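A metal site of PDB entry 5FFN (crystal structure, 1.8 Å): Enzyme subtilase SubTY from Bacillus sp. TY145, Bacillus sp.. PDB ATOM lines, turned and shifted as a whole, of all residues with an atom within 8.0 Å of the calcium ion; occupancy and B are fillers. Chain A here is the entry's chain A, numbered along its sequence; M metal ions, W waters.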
ATOM      1  N   ASN A 212     -22.099   4.929 -10.732  1.00  0.00           N
ATOM      2  CA  ASN A 212     -23.228   5.762 -11.092  1.00  0.00           C
ATOM      3  C   ASN A 212     -22.726   6.913 -11.990  1.00  0.00           C
ATOM      4  O   ASN A 212     -22.025   7.809 -11.525  1.00  0.00           O
ATOM      5  CB  ASN A 212     -23.857   6.283  -9.795  1.00  0.00           C
ATOM      6  CG  ASN A 212     -25.068   7.180 -10.042  1.00  0.00           C
ATOM      7  OD1 ASN A 212     -25.492   7.360 -11.173  1.00  0.00           O
ATOM      8  ND2 ASN A 212     -25.666   7.689  -8.966  1.00  0.00           N
ATOM      9  N   PRO A 213     -23.161   6.950 -13.282  1.00  0.00           N
ATOM     10  CA  PRO A 213     -22.684   8.078 -14.132  1.00  0.00           C
ATOM     11  C   PRO A 213     -22.941   9.468 -13.547  1.00  0.00           C
ATOM     12  O   PRO A 213     -22.083  10.359 -13.691  1.00  0.00           O
ATOM     13  CB  PRO A 213     -23.422   7.854 -15.457  1.00  0.00           C
ATOM     14  CG  PRO A 213     -23.695   6.398 -15.463  1.00  0.00           C
ATOM     15  CD  PRO A 213     -24.084   6.095 -14.039  1.00  0.00           C
ATOM     16  N   ALA A 214     -24.047   9.597 -12.805  1.00  0.00           N
ATOM     17  CA  ALA A 214     -24.516  10.868 -12.214  1.00  0.00           C
ATOM     18  C   ALA A 214     -23.520  11.460 -11.246  1.00  0.00           C
ATOM     19  O   ALA A 214     -23.518  12.675 -11.060  1.00  0.00           O
ATOM     20  CB  ALA A 214     -25.852  10.668 -11.506  1.00  0.00           C
ATOM     21  N   THR A 215     -22.649  10.633 -10.654  1.00  0.00           N
ATOM     22  CA  THR A 215     -21.728  11.132  -9.623  1.00  0.00           C
ATOM     23  C   THR A 215     -20.252  10.894  -9.925  1.00  0.00           C
ATOM     24  O   THR A 215     -19.412  11.097  -9.072  1.00  0.00           O
ATOM     25  CB  THR A 215     -22.107  10.549  -8.224  1.00  0.00           C
ATOM     26  OG1 THR A 215     -22.094   9.097  -8.242  1.00  0.00           O
ATOM     27  CG2 THR A 215     -23.445  11.038  -7.813  1.00  0.00           C
ATOM     28  N   ALA A 216     -19.950  10.506 -11.153  1.00  0.00           N
ATOM     29  CA  ALA A 216     -18.578  10.359 -11.611  1.00  0.00           C
ATOM     30  C   ALA A 216     -18.146  11.649 -12.299  1.00  0.00           C
ATOM     31  O   ALA A 216     -18.935  12.233 -13.039  1.00  0.00           O
ATOM     32  CB  ALA A 216     -18.433   9.188 -12.604  1.00  0.00           C
ATOM     33  N   GLY A 217     -16.900  12.055 -12.093  1.00  0.00           N
ATOM     34  CA  GLY A 217     -16.336  13.222 -12.757  1.00  0.00           C
ATOM     35  C   GLY A 217     -15.796  14.245 -11.768  1.00  0.00           C
ATOM     36  O   GLY A 217     -14.968  15.121 -12.155  1.00  0.00           O
ATOM     37  N   ASP A 218     -16.192  14.143 -10.511  1.00  0.00           N
ATOM     38  CA  ASP A 218     -15.825  15.142  -9.525  1.00  0.00           C
ATOM     39  C   ASP A 218     -14.570  14.843  -8.688  1.00  0.00           C
ATOM     40  O   ASP A 218     -14.071  15.714  -7.971  1.00  0.00           O
ATOM     41  CB  ASP A 218     -17.042  15.438  -8.648  1.00  0.00           C
ATOM     42  CG  ASP A 218     -17.538  14.228  -7.880  1.00  0.00           C
ATOM     43  OD1 ASP A 218     -17.065  13.086  -8.105  1.00  0.00           O
ATOM     44  OD2 ASP A 218     -18.470  14.443  -7.079  1.00  0.00           O
ATOM     45  N   TYR A 219     -13.980  13.672  -8.871  1.00  0.00           N
ATOM     46  CA  TYR A 219     -12.867  13.211  -8.033  1.00  0.00           C
ATOM     47  C   TYR A 219     -13.198  13.299  -6.514  1.00  0.00           C
ATOM     48  O   TYR A 219     -12.306  13.502  -5.689  1.00  0.00           O
ATOM     49  CB  TYR A 219     -11.580  13.973  -8.366  1.00  0.00           C
ATOM     50  CG  TYR A 219     -10.963  13.606  -9.699  1.00  0.00           C
ATOM     51  CD1 TYR A 219     -10.440  12.353  -9.922  1.00  0.00           C
ATOM     52  CD2 TYR A 219     -10.896  14.534 -10.719  1.00  0.00           C
ATOM     53  CE1 TYR A 219      -9.868  12.005 -11.141  1.00  0.00           C
ATOM     54  CE2 TYR A 219     -10.316  14.219 -11.922  1.00  0.00           C
ATOM     55  CZ  TYR A 219      -9.817  12.968 -12.140  1.00  0.00           C
ATOM     56  OH  TYR A 219      -9.216  12.739 -13.349  1.00  0.00           O
ATOM     57  N   ILE A 220     -14.460  13.076  -6.184  1.00  0.00           N
ATOM     58  CA  ILE A 220     -14.918  12.960  -4.817  1.00  0.00           C
ATOM     59  C   ILE A 220     -15.775  11.687  -4.738  1.00  0.00           C
ATOM     60  O   ILE A 220     -16.712  11.505  -5.500  1.00  0.00           O
ATOM     61  CB  ILE A 220     -15.739  14.171  -4.348  1.00  0.00           C
ATOM     62  CG1 ILE A 220     -14.871  15.435  -4.393  1.00  0.00           C
ATOM     63  CG2 ILE A 220     -16.267  13.951  -2.920  1.00  0.00           C
ATOM     64  CD1 ILE A 220     -15.685  16.685  -4.295  1.00  0.00           C
ATOM     65  N   ILE A 221     -15.427  10.825  -3.787  1.00  0.00           N
ATOM     66  CA  ILE A 221     -16.103   9.528  -3.682  1.00  0.00           C
ATOM     67  C   ILE A 221     -17.436   9.692  -2.932  1.00  0.00           C
ATOM     68  O   ILE A 221     -17.444  10.107  -1.731  1.00  0.00           O
ATOM     69  CB  ILE A 221     -15.193   8.486  -2.970  1.00  0.00           C
ATOM     70  CG1 ILE A 221     -13.965   8.159  -3.822  1.00  0.00           C
ATOM     71  CG2 ILE A 221     -15.966   7.243  -2.625  1.00  0.00           C
ATOM     72  CD1 ILE A 221     -14.259   7.581  -5.188  1.00  0.00           C
ATOM     73  N   GLN A 222     -18.536   9.388  -3.627  1.00  0.00           N
ATOM     74  CA  GLN A 222     -19.853   9.145  -3.058  1.00  0.00           C
ATOM     75  C   GLN A 222     -20.144   7.646  -3.099  1.00  0.00           C
ATOM     76  O   GLN A 222     -19.388   6.844  -3.682  1.00  0.00           O
ATOM     77  CB  GLN A 222     -20.964   9.934  -3.791  1.00  0.00           C
ATOM     78  CG  GLN A 222     -20.860  11.475  -3.641  1.00  0.00           C
ATOM     79  CD  GLN A 222     -19.940  12.168  -4.648  1.00  0.00           C
ATOM     80  OE1 GLN A 222     -19.789  11.726  -5.792  1.00  0.00           O
ATOM     81  NE2 GLN A 222     -19.332  13.283  -4.217  1.00  0.00           N
ATOM     82  N   GLU A 223     -21.195   7.240  -2.404  1.00  0.00           N
ATOM     83  CA  GLU A 223     -21.690   5.883  -2.546  1.00  0.00           C
ATOM     84  C   GLU A 223     -21.977   5.583  -4.031  1.00  0.00           C
ATOM     85  O   GLU A 223     -22.480   6.455  -4.747  1.00  0.00           O
ATOM     86  CB  GLU A 223     -22.938   5.706  -1.689  1.00  0.00           C
ATOM     87  CG  GLU A 223     -23.379   4.289  -1.557  1.00  0.00           C
ATOM     88  CD  GLU A 223     -24.424   4.132  -0.442  1.00  0.00           C
ATOM     89  OE1 GLU A 223     -24.063   3.773   0.690  1.00  0.00           O
ATOM     90  OE2 GLU A 223     -25.579   4.360  -0.754  1.00  0.00           O
ATOM     91  N   ARG A 224     -21.571   4.378  -4.470  1.00  0.00           N
ATOM     92  CA  ARG A 224     -21.764   3.863  -5.849  1.00  0.00           C
ATOM     93  C   ARG A 224     -20.706   4.443  -6.825  1.00  0.00           C
ATOM     94  O   ARG A 224     -20.854   4.305  -8.040  1.00  0.00           O
ATOM     95  CB  ARG A 224     -23.196   4.072  -6.371  1.00  0.00           C
ATOM     96  CG  ARG A 224     -24.297   3.546  -5.454  1.00  0.00           C
ATOM     97  CD  ARG A 224     -25.654   3.609  -6.181  1.00  0.00           C
ATOM     98  NE  ARG A 224     -25.765   2.578  -7.196  1.00  0.00           N
ATOM     99  CZ  ARG A 224     -26.156   1.325  -6.946  1.00  0.00           C
ATOM    100  NH1 ARG A 224     -26.506   0.938  -5.728  1.00  0.00           N
ATOM    101  NH2 ARG A 224     -26.184   0.445  -7.940  1.00  0.00           N
ATOM    102  N   ASP A 225     -19.603   4.993  -6.303  1.00  0.00           N
ATOM    103  CA  ASP A 225     -18.536   5.428  -7.175  1.00  0.00           C
ATOM    104  C   ASP A 225     -17.393   4.411  -7.190  1.00  0.00           C
ATOM    105  O   ASP A 225     -16.964   3.901  -6.137  1.00  0.00           O
ATOM    106  CB  ASP A 225     -17.926   6.757  -6.721  1.00  0.00           C
ATOM    107  CG  ASP A 225     -18.830   7.963  -6.955  1.00  0.00           C
ATOM    108  OD1 ASP A 225     -19.879   7.859  -7.595  1.00  0.00           O
ATOM    109  OD2 ASP A 225     -18.440   9.020  -6.438  1.00  0.00           O
ATOM    110  N   ILE A 226     -16.884   4.146  -8.380  1.00  0.00           N
ATOM    111  CA  ILE A 226     -15.643   3.385  -8.531  1.00  0.00           C
ATOM    112  C   ILE A 226     -14.484   4.276  -8.114  1.00  0.00           C
ATOM    113  O   ILE A 226     -14.469   5.468  -8.378  1.00  0.00           O
ATOM    114  CB  ILE A 226     -15.359   2.947 -10.036  1.00  0.00           C
ATOM    115  CG1 ILE A 226     -16.558   2.170 -10.566  1.00  0.00           C
ATOM    116  CG2 ILE A 226     -14.029   2.232 -10.191  1.00  0.00           C
ATOM    117  CD1 ILE A 226     -16.732   0.811  -9.882  1.00  0.00           C
ATOM    118  N   ASP A 299     -12.104  11.415 -14.191  1.00  0.00           N
ATOM    119  CA  ASP A 299     -12.817  10.496 -13.297  1.00  0.00           C
ATOM    120  C   ASP A 299     -14.023   9.979 -14.010  1.00  0.00           C
ATOM    121  O   ASP A 299     -14.844  10.773 -14.507  1.00  0.00           O
ATOM    122  CB  ASP A 299     -13.154  11.272 -12.038  1.00  0.00           C
ATOM    123  CG  ASP A 299     -14.038  10.529 -11.051  1.00  0.00           C
ATOM    124  OD1 ASP A 299     -13.940   9.307 -10.993  1.00  0.00           O
ATOM    125  OD2 ASP A 299     -14.809  11.239 -10.333  1.00  0.00           O
ATOM    126  N   PHE A 305     -10.875   6.979 -10.623  1.00  0.00           N
ATOM    127  CA  PHE A 305      -9.863   7.999 -10.693  1.00  0.00           C
ATOM    128  C   PHE A 305      -8.704   7.594 -11.579  1.00  0.00           C
ATOM    129  O   PHE A 305      -7.951   8.465 -12.012  1.00  0.00           O
ATOM    130  CB  PHE A 305      -9.271   8.321  -9.303  1.00  0.00           C
ATOM    131  CG  PHE A 305     -10.209   9.013  -8.319  1.00  0.00           C
ATOM    132  CD1 PHE A 305     -11.597   9.044  -8.486  1.00  0.00           C
ATOM    133  CD2 PHE A 305      -9.676   9.568  -7.152  1.00  0.00           C
ATOM    134  CE1 PHE A 305     -12.450   9.655  -7.529  1.00  0.00           C
ATOM    135  CE2 PHE A 305     -10.505  10.190  -6.222  1.00  0.00           C
ATOM    136  CZ  PHE A 305     -11.875  10.230  -6.393  1.00  0.00           C
HETATM  137 CA    CA M   1     -18.008  11.156  -7.274  1.00  0.00          CA
HETATM  138  O   HOH W   1     -16.304  10.146  -8.449  1.00  0.00           O
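The calcium ion is bound by O of Ile 220 (2.2 Å), O of Thr 215 (2.3 Å), OD1 of Asp 218 (2.3 Å), water W1 (2.3 Å), OD2 of Asp 225 (2.3 Å) and OE1 of Gln 222 (2.4 Å).
The calcium ion has six donor atoms within binding distance.
Within 4 Å of the calcium ion: Thr 215, Asp 218, Ile 220, Gln 222 and Asp 225.
The backbone NH of Asp 218 sits at hydrogen-bond distance from the side-chain carboxylate of Asp 299 (3.2 Å).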
